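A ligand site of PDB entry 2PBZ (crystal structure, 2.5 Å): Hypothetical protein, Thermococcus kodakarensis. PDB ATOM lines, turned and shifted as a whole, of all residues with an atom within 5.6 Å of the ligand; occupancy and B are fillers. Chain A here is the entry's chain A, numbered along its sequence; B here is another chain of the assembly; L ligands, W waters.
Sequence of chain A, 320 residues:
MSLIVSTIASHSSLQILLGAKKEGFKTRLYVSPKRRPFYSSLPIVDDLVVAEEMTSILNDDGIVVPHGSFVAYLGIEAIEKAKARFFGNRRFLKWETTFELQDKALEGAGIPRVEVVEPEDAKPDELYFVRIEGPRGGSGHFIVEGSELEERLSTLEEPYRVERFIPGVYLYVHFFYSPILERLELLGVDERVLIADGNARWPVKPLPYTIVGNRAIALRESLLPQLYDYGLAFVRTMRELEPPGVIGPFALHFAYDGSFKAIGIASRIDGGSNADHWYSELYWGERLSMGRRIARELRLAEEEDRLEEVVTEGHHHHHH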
ATOM      1  N   VAL A 114      26.407 -22.440 -10.489  1.00  0.00           N
ATOM      2  CA  VAL A 114      26.657 -21.734  -9.243  1.00  0.00           C
ATOM      3  C   VAL A 114      27.820 -20.807  -9.523  1.00  0.00           C
ATOM      4  O   VAL A 114      28.761 -21.177 -10.222  1.00  0.00           O
ATOM      5  CB  VAL A 114      27.070 -22.685  -8.125  1.00  0.00           C
ATOM      6  CG1 VAL A 114      25.902 -23.575  -7.774  1.00  0.00           C
ATOM      7  CG2 VAL A 114      28.269 -23.516  -8.551  1.00  0.00           C
ATOM      8  N   PHE A 129      31.249 -22.841  -0.124  1.00  0.00           N
ATOM      9  CA  PHE A 129      31.565 -24.237  -0.385  1.00  0.00           C
ATOM     10  C   PHE A 129      32.879 -24.275  -1.149  1.00  0.00           C
ATOM     11  O   PHE A 129      33.098 -23.485  -2.054  1.00  0.00           O
ATOM     12  CB  PHE A 129      30.450 -24.873  -1.236  1.00  0.00           C
ATOM     13  CG  PHE A 129      30.533 -26.380  -1.330  1.00  0.00           C
ATOM     14  CD1 PHE A 129      30.202 -27.186  -0.230  1.00  0.00           C
ATOM     15  CD2 PHE A 129      30.953 -26.994  -2.519  1.00  0.00           C
ATOM     16  CE1 PHE A 129      30.310 -28.583  -0.307  1.00  0.00           C
ATOM     17  CE2 PHE A 129      31.056 -28.396  -2.603  1.00  0.00           C
ATOM     18  CZ  PHE A 129      30.731 -29.184  -1.493  1.00  0.00           C
ATOM     19  N   ARG A 131      35.067 -26.693  -3.505  1.00  0.00           N
ATOM     20  CA  ARG A 131      34.998 -27.922  -4.299  1.00  0.00           C
ATOM     21  C   ARG A 131      36.366 -28.520  -4.594  1.00  0.00           C
ATOM     22  O   ARG A 131      37.366 -27.832  -4.508  1.00  0.00           O
ATOM     23  CB  ARG A 131      34.254 -27.659  -5.611  1.00  0.00           C
ATOM     24  CG  ARG A 131      33.882 -28.929  -6.354  1.00  0.00           C
ATOM     25  CD  ARG A 131      32.419 -29.314  -6.136  1.00  0.00           C
ATOM     26  NE  ARG A 131      31.550 -28.348  -6.795  1.00  0.00           N
ATOM     27  CZ  ARG A 131      31.585 -28.072  -8.096  1.00  0.00           C
ATOM     28  NH1 ARG A 131      32.473 -28.701  -8.879  1.00  0.00           N
ATOM     29  NH2 ARG A 131      30.758 -27.166  -8.629  1.00  0.00           N
ATOM     30  N   ILE A 132      36.368 -29.809  -4.956  1.00  0.00           N
ATOM     31  CA  ILE A 132      37.590 -30.577  -5.279  1.00  0.00           C
ATOM     32  C   ILE A 132      38.723 -30.350  -4.286  1.00  0.00           C
ATOM     33  O   ILE A 132      38.578 -30.629  -3.083  1.00  0.00           O
ATOM     34  CB  ILE A 132      38.129 -30.258  -6.703  1.00  0.00           C
ATOM     35  CG1 ILE A 132      37.173 -30.807  -7.771  1.00  0.00           C
ATOM     36  CG2 ILE A 132      39.530 -30.859  -6.894  1.00  0.00           C
ATOM     37  CD1 ILE A 132      37.780 -30.844  -9.173  1.00  0.00           C
ATOM     38  N   GLU A 145      35.523 -32.061  -0.085  1.00  0.00           N
ATOM     39  CA  GLU A 145      34.852 -30.768  -0.225  1.00  0.00           C
ATOM     40  C   GLU A 145      35.027 -30.021   1.089  1.00  0.00           C
ATOM     41  O   GLU A 145      36.142 -29.883   1.590  1.00  0.00           O
ATOM     42  CB  GLU A 145      33.354 -30.945  -0.549  1.00  0.00           C
ATOM     43  CG  GLU A 145      33.013 -32.199  -1.362  1.00  0.00           C
ATOM     44  CD  GLU A 145      33.273 -32.069  -2.847  1.00  0.00           C
ATOM     45  OE1 GLU A 145      34.293 -31.469  -3.248  1.00  0.00           O
ATOM     46  OE2 GLU A 145      32.439 -32.591  -3.627  1.00  0.00           O
ATOM     47  N   GLU A 163      32.717 -21.640  -3.990  1.00  0.00           N
ATOM     48  CA  GLU A 163      31.385 -21.324  -4.498  1.00  0.00           C
ATOM     49  C   GLU A 163      30.470 -20.786  -3.422  1.00  0.00           C
ATOM     50  O   GLU A 163      30.670 -21.051  -2.234  1.00  0.00           O
ATOM     51  CB  GLU A 163      30.751 -22.560  -5.159  1.00  0.00           C
ATOM     52  CG  GLU A 163      31.704 -23.300  -6.089  1.00  0.00           C
ATOM     53  CD  GLU A 163      31.046 -24.429  -6.864  1.00  0.00           C
ATOM     54  OE1 GLU A 163      30.360 -25.293  -6.251  1.00  0.00           O
ATOM     55  OE2 GLU A 163      31.225 -24.460  -8.112  1.00  0.00           O
ATOM     56  N   ARG A 164      29.487 -20.009  -3.858  1.00  0.00           N
ATOM     57  CA  ARG A 164      28.485 -19.421  -2.968  1.00  0.00           C
ATOM     58  C   ARG A 164      27.769 -20.585  -2.289  1.00  0.00           C
ATOM     59  O   ARG A 164      27.403 -21.551  -2.953  1.00  0.00           O
ATOM     60  CB  ARG A 164      27.498 -18.602  -3.794  1.00  0.00           C
ATOM     61  CG  ARG A 164      26.508 -17.749  -3.003  1.00  0.00           C
ATOM     62  CD  ARG A 164      27.202 -16.563  -2.355  1.00  0.00           C
ATOM     63  NE  ARG A 164      26.255 -15.587  -1.808  1.00  0.00           N
ATOM     64  CZ  ARG A 164      25.443 -15.805  -0.771  1.00  0.00           C
ATOM     65  NH1 ARG A 164      25.446 -16.985  -0.148  1.00  0.00           N
ATOM     66  NH2 ARG A 164      24.614 -14.839  -0.364  1.00  0.00           N
ATOM     67  N   PHE A 165      27.590 -20.508  -0.980  1.00  0.00           N
ATOM     68  CA  PHE A 165      26.900 -21.571  -0.279  1.00  0.00           C
ATOM     69  C   PHE A 165      25.419 -21.511  -0.606  1.00  0.00           C
ATOM     70  O   PHE A 165      24.791 -20.439  -0.507  1.00  0.00           O
ATOM     71  CB  PHE A 165      27.055 -21.427   1.225  1.00  0.00           C
ATOM     72  CG  PHE A 165      26.439 -22.545   2.004  1.00  0.00           C
ATOM     73  CD1 PHE A 165      27.189 -23.671   2.344  1.00  0.00           C
ATOM     74  CD2 PHE A 165      25.101 -22.490   2.406  1.00  0.00           C
ATOM     75  CE1 PHE A 165      26.638 -24.718   3.091  1.00  0.00           C
ATOM     76  CE2 PHE A 165      24.539 -23.529   3.153  1.00  0.00           C
ATOM     77  CZ  PHE A 165      25.313 -24.658   3.496  1.00  0.00           C
ATOM     78  N   ILE A 166      24.834 -22.640  -0.992  1.00  0.00           N
ATOM     79  CA  ILE A 166      23.418 -22.669  -1.320  1.00  0.00           C
ATOM     80  C   ILE A 166      22.709 -23.790  -0.567  1.00  0.00           C
ATOM     81  O   ILE A 166      23.039 -24.964  -0.750  1.00  0.00           O
ATOM     82  CB  ILE A 166      23.187 -22.873  -2.834  1.00  0.00           C
ATOM     83  CG1 ILE A 166      23.876 -21.755  -3.626  1.00  0.00           C
ATOM     84  CG2 ILE A 166      21.701 -22.899  -3.124  1.00  0.00           C
ATOM     85  CD1 ILE A 166      23.918 -22.013  -5.135  1.00  0.00           C
ATOM     86  N   PRO A 167      21.748 -23.445   0.308  1.00  0.00           N
ATOM     87  CA  PRO A 167      21.044 -24.491   1.045  1.00  0.00           C
ATOM     88  C   PRO A 167      19.779 -24.839   0.279  1.00  0.00           C
ATOM     89  O   PRO A 167      19.121 -23.938  -0.238  1.00  0.00           O
ATOM     90  CB  PRO A 167      20.731 -23.835   2.387  1.00  0.00           C
ATOM     91  CG  PRO A 167      21.538 -22.492   2.351  1.00  0.00           C
ATOM     92  CD  PRO A 167      21.486 -22.131   0.905  1.00  0.00           C
ATOM     93  N   TYR A 170      19.590 -30.975  -3.192  1.00  0.00           N
ATOM     94  CA  TYR A 170      20.480 -31.203  -4.311  1.00  0.00           C
ATOM     95  C   TYR A 170      19.930 -32.356  -5.117  1.00  0.00           C
ATOM     96  O   TYR A 170      19.752 -33.478  -4.621  1.00  0.00           O
ATOM     97  CB  TYR A 170      21.903 -31.473  -3.805  1.00  0.00           C
ATOM     98  CG  TYR A 170      22.565 -30.166  -3.453  1.00  0.00           C
ATOM     99  CD1 TYR A 170      22.138 -29.413  -2.371  1.00  0.00           C
ATOM    100  CD2 TYR A 170      23.533 -29.606  -4.307  1.00  0.00           C
ATOM    101  CE1 TYR A 170      22.635 -28.132  -2.135  1.00  0.00           C
ATOM    102  CE2 TYR A 170      24.023 -28.322  -4.083  1.00  0.00           C
ATOM    103  CZ  TYR A 170      23.572 -27.587  -3.002  1.00  0.00           C
ATOM    104  OH  TYR A 170      24.033 -26.306  -2.813  1.00  0.00           O
ATOM    105  N   TYR A 172      19.962 -34.740  -8.651  1.00  0.00           N
ATOM    106  CA  TYR A 172      20.808 -35.319  -9.661  1.00  0.00           C
ATOM    107  C   TYR A 172      19.930 -35.918 -10.751  1.00  0.00           C
ATOM    108  O   TYR A 172      19.345 -36.981 -10.592  1.00  0.00           O
ATOM    109  CB  TYR A 172      21.733 -36.351  -9.001  1.00  0.00           C
ATOM    110  CG  TYR A 172      22.557 -35.742  -7.888  1.00  0.00           C
ATOM    111  CD1 TYR A 172      21.953 -35.381  -6.687  1.00  0.00           C
ATOM    112  CD2 TYR A 172      23.896 -35.410  -8.079  1.00  0.00           C
ATOM    113  CE1 TYR A 172      22.668 -34.681  -5.697  1.00  0.00           C
ATOM    114  CE2 TYR A 172      24.617 -34.724  -7.096  1.00  0.00           C
ATOM    115  CZ  TYR A 172      23.997 -34.351  -5.908  1.00  0.00           C
ATOM    116  OH  TYR A 172      24.690 -33.632  -4.959  1.00  0.00           O
ATOM    117  N   ARG A 192      21.267 -37.530  -3.025  1.00  0.00           N
ATOM    118  CA  ARG A 192      22.349 -38.195  -2.307  1.00  0.00           C
ATOM    119  C   ARG A 192      22.121 -38.363  -0.799  1.00  0.00           C
ATOM    120  O   ARG A 192      21.487 -37.516  -0.149  1.00  0.00           O
ATOM    121  CB  ARG A 192      23.677 -37.446  -2.501  1.00  0.00           C
ATOM    122  CG  ARG A 192      24.039 -37.053  -3.919  1.00  0.00           C
ATOM    123  CD  ARG A 192      24.773 -38.149  -4.665  1.00  0.00           C
ATOM    124  NE  ARG A 192      24.114 -38.459  -5.933  1.00  0.00           N
ATOM    125  CZ  ARG A 192      24.679 -38.336  -7.128  1.00  0.00           C
ATOM    126  NH1 ARG A 192      25.930 -37.899  -7.236  1.00  0.00           N
ATOM    127  NH2 ARG A 192      23.987 -38.665  -8.202  1.00  0.00           N
ATOM    128  N   LEU A 194      24.237 -38.341   2.284  1.00  0.00           N
ATOM    129  CA  LEU A 194      25.555 -37.926   2.745  1.00  0.00           C
ATOM    130  C   LEU A 194      25.767 -38.233   4.211  1.00  0.00           C
ATOM    131  O   LEU A 194      24.798 -38.476   4.938  1.00  0.00           O
ATOM    132  CB  LEU A 194      25.741 -36.431   2.495  1.00  0.00           C
ATOM    133  CG  LEU A 194      26.252 -35.988   1.119  1.00  0.00           C
ATOM    134  CD1 LEU A 194      25.547 -36.755   0.023  1.00  0.00           C
ATOM    135  CD2 LEU A 194      26.030 -34.495   0.978  1.00  0.00           C
ATOM    136  N   TYR A 209      30.868 -34.332   3.094  1.00  0.00           N
ATOM    137  CA  TYR A 209      29.793 -34.520   2.122  1.00  0.00           C
ATOM    138  C   TYR A 209      29.935 -35.768   1.277  1.00  0.00           C
ATOM    139  O   TYR A 209      29.371 -35.859   0.193  1.00  0.00           O
ATOM    140  CB  TYR A 209      29.669 -33.298   1.229  1.00  0.00           C
ATOM    141  CG  TYR A 209      29.096 -32.115   1.972  1.00  0.00           C
ATOM    142  CD1 TYR A 209      29.894 -31.378   2.862  1.00  0.00           C
ATOM    143  CD2 TYR A 209      27.758 -31.762   1.830  1.00  0.00           C
ATOM    144  CE1 TYR A 209      29.353 -30.312   3.588  1.00  0.00           C
ATOM    145  CE2 TYR A 209      27.213 -30.702   2.549  1.00  0.00           C
ATOM    146  CZ  TYR A 209      28.005 -29.983   3.429  1.00  0.00           C
ATOM    147  OH  TYR A 209      27.432 -28.946   4.140  1.00  0.00           O
ATOM    148  N   HIS A 253      23.987 -32.042 -12.434  1.00  0.00           N
ATOM    149  CA  HIS A 253      23.836 -31.886 -10.994  1.00  0.00           C
ATOM    150  C   HIS A 253      23.373 -30.472 -10.649  1.00  0.00           C
ATOM    151  O   HIS A 253      23.939 -29.486 -11.133  1.00  0.00           O
ATOM    152  CB  HIS A 253      25.163 -32.231 -10.301  1.00  0.00           C
ATOM    153  CG  HIS A 253      25.649 -33.629 -10.603  1.00  0.00           C
ATOM    154  ND1 HIS A 253      26.871 -34.094 -10.184  1.00  0.00           N
ATOM    155  CD2 HIS A 253      25.056 -34.644 -11.266  1.00  0.00           C
ATOM    156  CE1 HIS A 253      27.025 -35.352 -10.585  1.00  0.00           C
ATOM    157  NE2 HIS A 253      25.940 -35.702 -11.250  1.00  0.00           N
ATOM    158  N   ILE A 263      25.873 -27.423 -10.639  1.00  0.00           N
ATOM    159  CA  ILE A 263      27.069 -27.549  -9.825  1.00  0.00           C
ATOM    160  C   ILE A 263      28.022 -28.551 -10.464  1.00  0.00           C
ATOM    161  O   ILE A 263      29.199 -28.596 -10.112  1.00  0.00           O
ATOM    162  CB  ILE A 263      26.749 -28.024  -8.386  1.00  0.00           C
ATOM    163  CG1 ILE A 263      26.017 -29.363  -8.422  1.00  0.00           C
ATOM    164  CG2 ILE A 263      25.947 -26.981  -7.659  1.00  0.00           C
ATOM    165  CD1 ILE A 263      26.024 -30.109  -7.098  1.00  0.00           C
ATOM    166  N   ARG B 201      21.965 -30.871   6.255  1.00  0.00           N
ATOM    167  CA  ARG B 201      23.414 -31.072   6.214  1.00  0.00           C
ATOM    168  C   ARG B 201      24.054 -30.091   7.197  1.00  0.00           C
ATOM    169  O   ARG B 201      24.894 -30.470   7.999  1.00  0.00           O
ATOM    170  CB  ARG B 201      23.957 -30.782   4.821  1.00  0.00           C
ATOM    171  CG  ARG B 201      23.197 -31.401   3.679  1.00  0.00           C
ATOM    172  CD  ARG B 201      23.515 -32.862   3.448  1.00  0.00           C
ATOM    173  NE  ARG B 201      23.171 -33.187   2.069  1.00  0.00           N
ATOM    174  CZ  ARG B 201      22.791 -34.388   1.645  1.00  0.00           C
ATOM    175  NH1 ARG B 201      22.682 -35.391   2.515  1.00  0.00           N
ATOM    176  NH2 ARG B 201      22.502 -34.564   0.359  1.00  0.00           N
HETATM  177  P1  LIG L   1      33.448 -35.556  -6.684  1.00  0.00           P
HETATM  178  O1  LIG L   1      33.798 -34.477  -7.703  1.00  0.00           O
HETATM  179  O2  LIG L   1      34.859 -36.126  -6.015  1.00  0.00           O
HETATM  180  O3  LIG L   1      32.652 -36.791  -7.415  1.00  0.00           O
HETATM  181  P2  LIG L   1      31.083 -34.351  -6.147  1.00  0.00           P
HETATM  182  O4  LIG L   1      31.373 -33.279  -7.127  1.00  0.00           O
HETATM  183  O5  LIG L   1      30.264 -35.558  -6.858  1.00  0.00           O
HETATM  184  O6  LIG L   1      32.485 -34.920  -5.515  1.00  0.00           O
HETATM  185  P3  LIG L   1      28.776 -33.109  -5.145  1.00  0.00           P
HETATM  186  O7  LIG L   1      27.825 -34.051  -5.779  1.00  0.00           O
HETATM  187  O8  LIG L   1      28.923 -31.775  -6.027  1.00  0.00           O
HETATM  188  O9  LIG L   1      30.268 -33.780  -4.867  1.00  0.00           O
HETATM  189  O10 LIG L   1      28.315 -32.764  -3.637  1.00  0.00           O
HETATM  190  C1  LIG L   1      27.018 -32.259  -3.586  1.00  0.00           C
HETATM  191  C2  LIG L   1      26.771 -32.042  -2.095  1.00  0.00           C
HETATM  192  O11 LIG L   1      27.712 -31.079  -1.523  1.00  0.00           O
HETATM  193  C3  LIG L   1      25.347 -31.550  -1.815  1.00  0.00           C
HETATM  194  O12 LIG L   1      24.688 -32.505  -1.019  1.00  0.00           O
HETATM  195  C4  LIG L   1      25.483 -30.224  -1.113  1.00  0.00           C
HETATM  196  O13 LIG L   1      24.912 -30.301   0.215  1.00  0.00           O
HETATM  197  C5  LIG L   1      26.988 -29.902  -1.081  1.00  0.00           C
HETATM  198  N1  LIG L   1      27.214 -28.751  -1.973  1.00  0.00           N
HETATM  199  C6  LIG L   1      27.716 -28.761  -3.255  1.00  0.00           C
HETATM  200  N2  LIG L   1      27.779 -27.568  -3.736  1.00  0.00           N
HETATM  201  C7  LIG L   1      27.322 -26.694  -2.801  1.00  0.00           C
HETATM  202  C8  LIG L   1      27.149 -25.277  -2.742  1.00  0.00           C
HETATM  203  N3  LIG L   1      27.502 -24.488  -3.841  1.00  0.00           N
HETATM  204  N4  LIG L   1      26.641 -24.716  -1.587  1.00  0.00           N
HETATM  205  C9  LIG L   1      26.303 -25.463  -0.525  1.00  0.00           C
HETATM  206  N5  LIG L   1      26.452 -26.797  -0.549  1.00  0.00           N
HETATM  207  C10 LIG L   1      26.954 -27.433  -1.648  1.00  0.00           C
HETATM  208  O   HOH W   1      31.610 -36.076  -2.724  1.00  0.00           O
HETATM  209  O   HOH W   2      29.168 -29.115  -6.763  1.00  0.00           O
HETATM  210  O   HOH W   3      34.602 -37.887  -3.941  1.00  0.00           O
HETATM  211  O   HOH W   4      29.560 -37.215  -9.038  1.00  0.00           O
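N4 of the ligand lies close to OH of Tyr 170. O of Arg 164 lies within hydrogen-bond range of N3 of the ligand. OH of Tyr 172 sits close to O7 of the ligand (3.3 Å). The guanidinium group (NH2) of Arg 201 of chain B lies within hydrogen-bond range of an oxygen (O12) of the ligand (3.3 Å). A nitrogen (N4) of the ligand sits at hydrogen-bond distance from the backbone NH (N) of Ile 166, 2.8 Å away.
N of Ile 263 is in hydrogen-bond range of O of His 253. The backbone carbonyl oxygen (O) of Ile 263 is in hydrogen-bond range of the guanidinium group (NH2) of Arg 131, 2.6 Å away. The backbone carbonyl oxygen (O) of Phe 129 is in hydrogen-bond range of the backbone NH (N) of Glu 163 (2.7 Å). The side-chain carboxylate of Glu 145 lies within hydrogen-bond range of the backbone NH of Ile 132, 3.2 Å away. OH of Tyr 170 is in hydrogen-bond range of O of Ile 166. NH2 of Arg 131 lies within salt-bridge range of OE2 of Glu 163 (2.8 Å). NH2 of Arg 201 of chain B lies within hydrogen-bond range of O of Arg 192 (3.2 Å).
O9 of the ligand sits close to OE2 of Glu 145 (2.8 Å). Residues that only touch the ligand: Leu 194, Tyr 209, Phe 165, Phe 129, Ile 263 and Glu 163. Hydrophobic or aromatic side chains within 4 Å of the ligand: Phe 129, Phe 165, Tyr 170, Tyr 172, Leu 194, Tyr 209 and Ile 263. Of the 18 residues printed, 12 come within 4 Å of the ligand.
Water W2 lies within hydrogen-bond range of the guanidinium group (NE) of Arg 131 (2.5 Å), an oxygen (O8) of the ligand (2.8 Å) and the backbone carbonyl oxygen (O) of Ile 263 (3.4 Å).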
